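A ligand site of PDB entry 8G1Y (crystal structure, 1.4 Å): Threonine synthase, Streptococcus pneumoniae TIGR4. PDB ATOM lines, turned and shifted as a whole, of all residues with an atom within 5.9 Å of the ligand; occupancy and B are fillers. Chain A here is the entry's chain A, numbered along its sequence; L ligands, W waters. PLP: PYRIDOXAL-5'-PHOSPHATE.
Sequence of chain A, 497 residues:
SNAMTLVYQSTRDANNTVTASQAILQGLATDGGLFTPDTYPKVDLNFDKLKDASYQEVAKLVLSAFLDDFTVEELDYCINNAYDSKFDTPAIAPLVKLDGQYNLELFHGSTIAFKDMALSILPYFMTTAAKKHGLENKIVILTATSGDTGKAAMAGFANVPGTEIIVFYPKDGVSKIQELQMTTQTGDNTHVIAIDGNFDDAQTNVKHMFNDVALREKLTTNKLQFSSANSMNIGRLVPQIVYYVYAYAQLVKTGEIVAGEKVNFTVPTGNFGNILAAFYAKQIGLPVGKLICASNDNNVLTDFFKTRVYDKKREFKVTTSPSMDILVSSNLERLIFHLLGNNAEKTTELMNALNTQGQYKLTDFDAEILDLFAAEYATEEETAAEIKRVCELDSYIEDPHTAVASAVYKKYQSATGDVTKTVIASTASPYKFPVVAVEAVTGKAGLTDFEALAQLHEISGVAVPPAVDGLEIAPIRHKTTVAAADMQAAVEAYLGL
The side-chain amino group of Lys 115 is covalently linked to a carbon (C4A) of the ligand (1.3 Å). The side-chain carboxylate (OD2) of Asp 148 lies close to an oxygen (O3) of the ligand, 2.4 Å away. The backbone NH (N) of Gly 270 sits close to an oxygen (O1P) of the ligand (2.7 Å). N of Asn 271 lies close to O3P of the ligand. OG1 of Thr 427 lies close to N1 of the ligand, 2.9 Å away. An oxygen (O2P) of the ligand lies close to the backbone NH (N) of Asn 274. O1P of the ligand sits close to N of Phe 272, 3.0 Å away. An oxygen (O3) of the ligand sits close to the side-chain hydroxyl (OG) of Ser 323 (3.4 Å). N of Gly 273 sits close to O2P of the ligand (3.4 Å).
Water W4 lies within hydrogen-bond range of N of Lys 115 (3.0 Å), N of Phe 114 (3.4 Å) and OD2 of Asp 148 (3.5 Å). Water W2 lies within hydrogen-bond range of N of Ile 275, OG1 of Thr 269 and N of Asn 274. Water W1 lies within hydrogen-bond range of the backbone carbonyl oxygen (O) of Pro 268 (2.6 Å) and the side-chain amide nitrogen (ND2) of Asn 274 (2.8 Å). Water W5 bridges O of Ser 323 and NZ of Lys 115.
Merely in contact with the ligand: Phe 114, Thr 269, Pro 268, Ala 428, His 401 and Met 324. Hydrophobic or aromatic side chains within 4 Å of the ligand: Phe 114, Met 324, His 401 and Ala 428. The nearest printed residue that does not touch the ligand is Phe 433 (4.5 Å).
The side-chain amino group (NZ) of Lys 115 is in salt-bridge range of the side-chain carboxylate (OD1) of Asp 148. OG of Ser 323 is in hydrogen-bond range of OD2 of Asp 148 (2.9 Å). N of Asn 331 sits at hydrogen-bond distance from O of Asn 271. The backbone carbonyl oxygen of Thr 427 sits at hydrogen-bond distance from the backbone NH of Phe 114. The backbone NH (N) of Ser 323 is in hydrogen-bond range of a ring nitrogen (NE2) of His 401 (3.0 Å). The backbone carbonyl oxygen (O) of Gly 273 sits at hydrogen-bond distance from the side-chain amide nitrogen (NE2) of Gln 240 (3.4 Å). OG1 of Thr 269 is in hydrogen-bond range of O of Val 267. ND1 of His 401 lies within hydrogen-bond range of OD2 of Asp 399 (2.8 Å).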
ATOM      1  N   ALA A 113       7.830  11.383  17.418  1.00  0.00           N
ATOM      2  CA  ALA A 113       8.462  12.110  16.291  1.00  0.00           C
ATOM      3  C   ALA A 113       9.903  12.440  16.700  1.00  0.00           C
ATOM      4  O   ALA A 113      10.145  12.650  17.889  1.00  0.00           O
ATOM      5  CB  ALA A 113       7.659  13.320  15.919  1.00  0.00           C
ATOM      6  N   PHE A 114      10.818  12.514  15.739  1.00  0.00           N
ATOM      7  CA  PHE A 114      12.257  12.609  16.092  1.00  0.00           C
ATOM      8  C   PHE A 114      12.609  13.929  16.790  1.00  0.00           C
ATOM      9  O   PHE A 114      13.662  13.959  17.417  1.00  0.00           O
ATOM     10  CB  PHE A 114      13.138  12.403  14.859  1.00  0.00           C
ATOM     11  CG  PHE A 114      13.531  13.675  14.160  1.00  0.00           C
ATOM     12  CD1 PHE A 114      12.668  14.344  13.312  1.00  0.00           C
ATOM     13  CD2 PHE A 114      14.795  14.210  14.362  1.00  0.00           C
ATOM     14  CE1 PHE A 114      13.055  15.511  12.691  1.00  0.00           C
ATOM     15  CE2 PHE A 114      15.183  15.386  13.747  1.00  0.00           C
ATOM     16  CZ  PHE A 114      14.308  16.037  12.911  1.00  0.00           C
ATOM     17  N   LYS A 115      11.768  14.951  16.699  1.00  0.00           N
ATOM     18  CA  LYS A 115      12.119  16.238  17.355  1.00  0.00           C
ATOM     19  C   LYS A 115      12.172  16.016  18.862  1.00  0.00           C
ATOM     20  O   LYS A 115      12.800  16.815  19.559  1.00  0.00           O
ATOM     21  CB  LYS A 115      11.178  17.354  16.922  1.00  0.00           C
ATOM     22  CG  LYS A 115      11.357  17.808  15.486  1.00  0.00           C
ATOM     23  CD  LYS A 115      10.435  18.921  15.076  1.00  0.00           C
ATOM     24  CE  LYS A 115      10.589  19.333  13.636  1.00  0.00           C
ATOM     25  NZ  LYS A 115      10.118  18.272  12.712  1.00  0.00           N
ATOM     26  N   ASP A 148       4.700  19.638  13.891  1.00  0.00           N
ATOM     27  CA  ASP A 148       4.792  18.741  15.079  1.00  0.00           C
ATOM     28  C   ASP A 148       5.738  19.333  16.126  1.00  0.00           C
ATOM     29  O   ASP A 148       5.791  18.783  17.244  1.00  0.00           O
ATOM     30  CB  ASP A 148       5.208  17.322  14.652  1.00  0.00           C
ATOM     31  CG  ASP A 148       6.406  17.245  13.733  1.00  0.00           C
ATOM     32  OD1 ASP A 148       7.184  18.247  13.658  1.00  0.00           O
ATOM     33  OD2 ASP A 148       6.545  16.185  13.049  1.00  0.00           O
ATOM     34  N   THR A 149       6.450  20.407  15.782  1.00  0.00           N
ATOM     35  CA  THR A 149       7.376  21.039  16.745  1.00  0.00           C
ATOM     36  C   THR A 149       6.595  21.513  17.984  1.00  0.00           C
ATOM     37  O   THR A 149       7.120  21.403  19.069  1.00  0.00           O
ATOM     38  CB  THR A 149       8.137  22.221  16.133  1.00  0.00           C
ATOM     39  OG1 THR A 149       8.854  21.764  14.990  1.00  0.00           O
ATOM     40  CG2 THR A 149       9.093  22.859  17.103  1.00  0.00           C
ATOM     41  N   SER A 231      14.093  25.933  15.145  1.00  0.00           N
ATOM     42  CA  SER A 231      14.941  25.024  14.336  1.00  0.00           C
ATOM     43  C   SER A 231      16.416  25.421  14.333  1.00  0.00           C
ATOM     44  O   SER A 231      17.253  24.591  14.001  1.00  0.00           O
ATOM     45  CB  SER A 231      14.429  24.972  12.914  1.00  0.00           C
ATOM     46  OG  SER A 231      14.596  26.236  12.275  1.00  0.00           O
ATOM     47  N   GLN A 240      21.277  15.544  17.969  1.00  0.00           N
ATOM     48  CA  GLN A 240      20.916  14.697  16.789  1.00  0.00           C
ATOM     49  C   GLN A 240      22.175  14.010  16.243  1.00  0.00           C
ATOM     50  O   GLN A 240      22.023  12.978  15.586  1.00  0.00           O
ATOM     51  CB  GLN A 240      20.186  15.551  15.751  1.00  0.00           C
ATOM     52  CG  GLN A 240      18.887  16.081  16.329  1.00  0.00           C
ATOM     53  CD  GLN A 240      18.039  16.963  15.457  1.00  0.00           C
ATOM     54  OE1 GLN A 240      16.886  17.207  15.793  1.00  0.00           O
ATOM     55  NE2 GLN A 240      18.587  17.501  14.384  1.00  0.00           N
ATOM     56  N   VAL A 267      17.882  10.965   4.748  1.00  0.00           N
ATOM     57  CA  VAL A 267      17.185  11.742   5.801  1.00  0.00           C
ATOM     58  C   VAL A 267      16.027  12.518   5.201  1.00  0.00           C
ATOM     59  O   VAL A 267      16.252  13.343   4.313  1.00  0.00           O
ATOM     60  CB  VAL A 267      18.174  12.699   6.484  1.00  0.00           C
ATOM     61  CG1 VAL A 267      17.533  13.411   7.658  1.00  0.00           C
ATOM     62  CG2 VAL A 267      19.438  11.960   6.910  1.00  0.00           C
ATOM     63  N   PRO A 268      14.784  12.297   5.685  1.00  0.00           N
ATOM     64  CA  PRO A 268      13.623  13.070   5.268  1.00  0.00           C
ATOM     65  C   PRO A 268      13.896  14.483   5.779  1.00  0.00           C
ATOM     66  O   PRO A 268      13.951  14.665   6.998  1.00  0.00           O
ATOM     67  CB  PRO A 268      12.402  12.402   5.914  1.00  0.00           C
ATOM     68  CG  PRO A 268      12.944  11.295   6.791  1.00  0.00           C
ATOM     69  CD  PRO A 268      14.452  11.319   6.726  1.00  0.00           C
ATOM     70  N   THR A 269      14.047  15.444   4.867  1.00  0.00           N
ATOM     71  CA  THR A 269      14.589  16.765   5.264  1.00  0.00           C
ATOM     72  C   THR A 269      13.573  17.889   5.083  1.00  0.00           C
ATOM     73  O   THR A 269      12.887  17.945   4.051  1.00  0.00           O
ATOM     74  CB  THR A 269      15.884  17.024   4.495  1.00  0.00           C
ATOM     75  OG1 THR A 269      16.840  16.051   4.920  1.00  0.00           O
ATOM     76  CG2 THR A 269      16.435  18.413   4.699  1.00  0.00           C
ATOM     77  N   GLY A 270      13.544  18.762   6.090  1.00  0.00           N
ATOM     78  CA  GLY A 270      12.731  19.992   6.077  1.00  0.00           C
ATOM     79  C   GLY A 270      13.665  21.180   6.259  1.00  0.00           C
ATOM     80  O   GLY A 270      14.151  21.735   5.246  1.00  0.00           O
ATOM     81  N   ASN A 271      13.982  21.480   7.522  1.00  0.00           N
ATOM     82  CA  ASN A 271      14.892  22.616   7.834  1.00  0.00           C
ATOM     83  C   ASN A 271      16.374  22.200   7.905  1.00  0.00           C
ATOM     84  O   ASN A 271      17.177  23.036   8.284  1.00  0.00           O
ATOM     85  CB  ASN A 271      14.413  23.361   9.071  1.00  0.00           C
ATOM     86  CG  ASN A 271      13.214  24.204   8.737  1.00  0.00           C
ATOM     87  OD1 ASN A 271      13.283  25.096   7.893  1.00  0.00           O
ATOM     88  ND2 ASN A 271      12.097  23.927   9.379  1.00  0.00           N
ATOM     89  N   PHE A 272      16.697  20.928   7.634  1.00  0.00           N
ATOM     90  CA  PHE A 272      18.099  20.509   7.366  1.00  0.00           C
ATOM     91  C   PHE A 272      18.913  20.189   8.633  1.00  0.00           C
ATOM     92  O   PHE A 272      20.049  19.708   8.482  1.00  0.00           O
ATOM     93  CB  PHE A 272      18.821  21.556   6.496  1.00  0.00           C
ATOM     94  CG  PHE A 272      19.881  20.965   5.596  1.00  0.00           C
ATOM     95  CD1 PHE A 272      19.538  20.370   4.402  1.00  0.00           C
ATOM     96  CD2 PHE A 272      21.226  21.017   5.935  1.00  0.00           C
ATOM     97  CE1 PHE A 272      20.505  19.810   3.579  1.00  0.00           C
ATOM     98  CE2 PHE A 272      22.193  20.452   5.121  1.00  0.00           C
ATOM     99  CZ  PHE A 272      21.829  19.854   3.934  1.00  0.00           C
ATOM    100  N   GLY A 273      18.377  20.397   9.840  1.00  0.00           N
ATOM    101  CA  GLY A 273      19.197  20.095  11.036  1.00  0.00           C
ATOM    102  C   GLY A 273      19.509  18.616  11.213  1.00  0.00           C
ATOM    103  O   GLY A 273      20.591  18.291  11.730  1.00  0.00           O
ATOM    104  N   ASN A 274      18.614  17.738  10.798  1.00  0.00           N
ATOM    105  CA  ASN A 274      18.816  16.279  10.996  1.00  0.00           C
ATOM    106  C   ASN A 274      19.971  15.822  10.094  1.00  0.00           C
ATOM    107  O   ASN A 274      20.941  15.195  10.583  1.00  0.00           O
ATOM    108  CB  ASN A 274      17.502  15.537  10.736  1.00  0.00           C
ATOM    109  CG  ASN A 274      17.446  14.152  11.330  1.00  0.00           C
ATOM    110  OD1 ASN A 274      18.366  13.716  11.994  1.00  0.00           O
ATOM    111  ND2 ASN A 274      16.350  13.464  11.070  1.00  0.00           N
ATOM    112  N   ILE A 275      19.918  16.177   8.815  1.00  0.00           N
ATOM    113  CA  ILE A 275      21.006  15.738   7.892  1.00  0.00           C
ATOM    114  C   ILE A 275      22.288  16.509   8.223  1.00  0.00           C
ATOM    115  O   ILE A 275      23.397  15.946   8.057  1.00  0.00           O
ATOM    116  CB  ILE A 275      20.569  15.885   6.420  1.00  0.00           C
ATOM    117  CG1 ILE A 275      21.530  15.120   5.511  1.00  0.00           C
ATOM    118  CG2 ILE A 275      20.419  17.336   6.014  1.00  0.00           C
ATOM    119  CD1 ILE A 275      21.053  15.019   4.088  1.00  0.00           C
ATOM    120  N   SER A 323       5.705  17.794   7.629  1.00  0.00           N
ATOM    121  CA  SER A 323       6.868  18.349   8.378  1.00  0.00           C
ATOM    122  C   SER A 323       7.980  18.758   7.417  1.00  0.00           C
ATOM    123  O   SER A 323       8.941  19.408   7.835  1.00  0.00           O
ATOM    124  CB  SER A 323       7.372  17.358   9.400  1.00  0.00           C
ATOM    125  OG  SER A 323       6.317  16.933  10.243  1.00  0.00           O
ATOM    126  N   MET A 324       7.857  18.376   6.130  1.00  0.00           N
ATOM    127  CA  MET A 324       8.881  18.710   5.149  1.00  0.00           C
ATOM    128  C   MET A 324       8.378  19.715   4.124  1.00  0.00           C
ATOM    129  O   MET A 324       9.051  19.952   3.112  1.00  0.00           O
ATOM    130  CB  MET A 324       9.367  17.419   4.479  1.00  0.00           C
ATOM    131  CG  MET A 324       9.998  16.462   5.467  1.00  0.00           C
ATOM    132  SD  MET A 324       9.940  14.629   4.832  1.00  0.00           S
ATOM    133  CE  MET A 324      10.979  14.970   3.286  1.00  0.00           C
ATOM    134  N   ASN A 331      18.420  25.501   8.318  1.00  0.00           N
ATOM    135  CA  ASN A 331      19.802  25.082   8.701  1.00  0.00           C
ATOM    136  C   ASN A 331      20.674  24.891   7.464  1.00  0.00           C
ATOM    137  O   ASN A 331      21.877  24.657   7.653  1.00  0.00           O
ATOM    138  CB  ASN A 331      19.755  23.879   9.635  1.00  0.00           C
ATOM    139  CG  ASN A 331      19.190  24.273  10.983  1.00  0.00           C
ATOM    140  OD1 ASN A 331      19.755  25.135  11.662  1.00  0.00           O
ATOM    141  ND2 ASN A 331      18.065  23.696  11.366  1.00  0.00           N
ATOM    142  N   ASP A 399       5.848   5.578   8.352  1.00  0.00           N
ATOM    143  CA  ASP A 399       5.051   6.826   8.270  1.00  0.00           C
ATOM    144  C   ASP A 399       5.366   7.476   6.919  1.00  0.00           C
ATOM    145  O   ASP A 399       6.334   7.098   6.261  1.00  0.00           O
ATOM    146  CB  ASP A 399       5.370   7.749   9.444  1.00  0.00           C
ATOM    147  CG  ASP A 399       6.303   8.895   9.088  1.00  0.00           C
ATOM    148  OD1 ASP A 399       7.498   8.634   8.853  1.00  0.00           O
ATOM    149  OD2 ASP A 399       5.787  10.029   8.987  1.00  0.00           O
ATOM    150  N   HIS A 401       6.726  10.473   6.160  1.00  0.00           N
ATOM    151  CA  HIS A 401       8.055  11.152   6.071  1.00  0.00           C
ATOM    152  C   HIS A 401       9.144  10.096   5.836  1.00  0.00           C
ATOM    153  O   HIS A 401      10.004  10.277   4.954  1.00  0.00           O
ATOM    154  CB  HIS A 401       8.311  12.000   7.321  1.00  0.00           C
ATOM    155  CG  HIS A 401       7.257  13.020   7.575  1.00  0.00           C
ATOM    156  ND1 HIS A 401       6.112  12.731   8.299  1.00  0.00           N
ATOM    157  CD2 HIS A 401       7.157  14.318   7.225  1.00  0.00           C
ATOM    158  CE1 HIS A 401       5.359  13.814   8.371  1.00  0.00           C
ATOM    159  NE2 HIS A 401       5.969  14.802   7.732  1.00  0.00           N
ATOM    160  N   THR A 427      11.594   9.394  10.928  1.00  0.00           N
ATOM    161  CA  THR A 427      11.320  10.597  11.759  1.00  0.00           C
ATOM    162  C   THR A 427       9.986  10.594  12.476  1.00  0.00           C
ATOM    163  O   THR A 427       9.824  11.464  13.347  1.00  0.00           O
ATOM    164  CB  THR A 427      11.549  11.827  10.875  1.00  0.00           C
ATOM    165  OG1 THR A 427      10.744  11.634   9.707  1.00  0.00           O
ATOM    166  CG2 THR A 427      13.000  11.980  10.482  1.00  0.00           C
ATOM    167  N   ALA A 428       9.071   9.693  12.161  1.00  0.00           N
ATOM    168  CA  ALA A 428       7.808   9.635  12.923  1.00  0.00           C
ATOM    169  C   ALA A 428       7.237   8.230  12.847  1.00  0.00           C
ATOM    170  O   ALA A 428       7.567   7.487  11.919  1.00  0.00           O
ATOM    171  CB  ALA A 428       6.800  10.633  12.402  1.00  0.00           C
ATOM    172  N   PHE A 433       0.729   9.941  11.749  1.00  0.00           N
ATOM    173  CA  PHE A 433       0.137  10.340  10.441  1.00  0.00           C
ATOM    174  C   PHE A 433      -0.597   9.120   9.915  1.00  0.00           C
ATOM    175  O   PHE A 433      -0.287   8.587   8.851  1.00  0.00           O
ATOM    176  CB  PHE A 433       1.238  10.843   9.498  1.00  0.00           C
ATOM    177  CG  PHE A 433       2.033  11.992  10.058  1.00  0.00           C
ATOM    178  CD1 PHE A 433       1.553  13.286   9.997  1.00  0.00           C
ATOM    179  CD2 PHE A 433       3.240  11.779  10.703  1.00  0.00           C
ATOM    180  CE1 PHE A 433       2.246  14.336  10.557  1.00  0.00           C
ATOM    181  CE2 PHE A 433       3.943  12.832  11.278  1.00  0.00           C
ATOM    182  CZ  PHE A 433       3.442  14.111  11.205  1.00  0.00           C
HETATM  183  N1  PLP L   1      10.121  14.411   9.480  1.00  0.00           N
HETATM  184  C2  PLP L   1       9.406  14.672  10.579  1.00  0.00           C
HETATM  185  C2A PLP L   1       8.401  13.661  11.051  1.00  0.00           C
HETATM  186  C3  PLP L   1       9.594  15.873  11.281  1.00  0.00           C
HETATM  187  O3  PLP L   1       8.864  16.095  12.391  1.00  0.00           O
HETATM  188  C4  PLP L   1      10.540  16.805  10.814  1.00  0.00           C
HETATM  189  C4A PLP L   1      10.751  18.055  11.547  1.00  0.00           C
HETATM  190  C5  PLP L   1      11.285  16.504   9.660  1.00  0.00           C
HETATM  191  C6  PLP L   1      11.031  15.303   9.043  1.00  0.00           C
HETATM  192  C5A PLP L   1      12.319  17.455   9.110  1.00  0.00           C
HETATM  193  O4P PLP L   1      13.515  17.540   9.962  1.00  0.00           O
HETATM  194  P   PLP L   1      14.708  18.642   9.707  1.00  0.00           P
HETATM  195  O1P PLP L   1      15.123  18.474   8.251  1.00  0.00           O
HETATM  196  O2P PLP L   1      15.811  18.305  10.673  1.00  0.00           O
HETATM  197  O3P PLP L   1      14.021  19.972   9.943  1.00  0.00           O
HETATM  198  O   HOH W   1      14.515  14.926   9.574  1.00  0.00           O
HETATM  199  O   HOH W   2      17.373  17.067   7.700  1.00  0.00           O
HETATM  200  O   HOH W   3      12.027  21.397  10.944  1.00  0.00           O
HETATM  201  O   HOH W   4       9.421  15.521  14.921  1.00  0.00           O
HETATM  202  O   HOH W   5       9.408  20.641  10.256  1.00  0.00           O
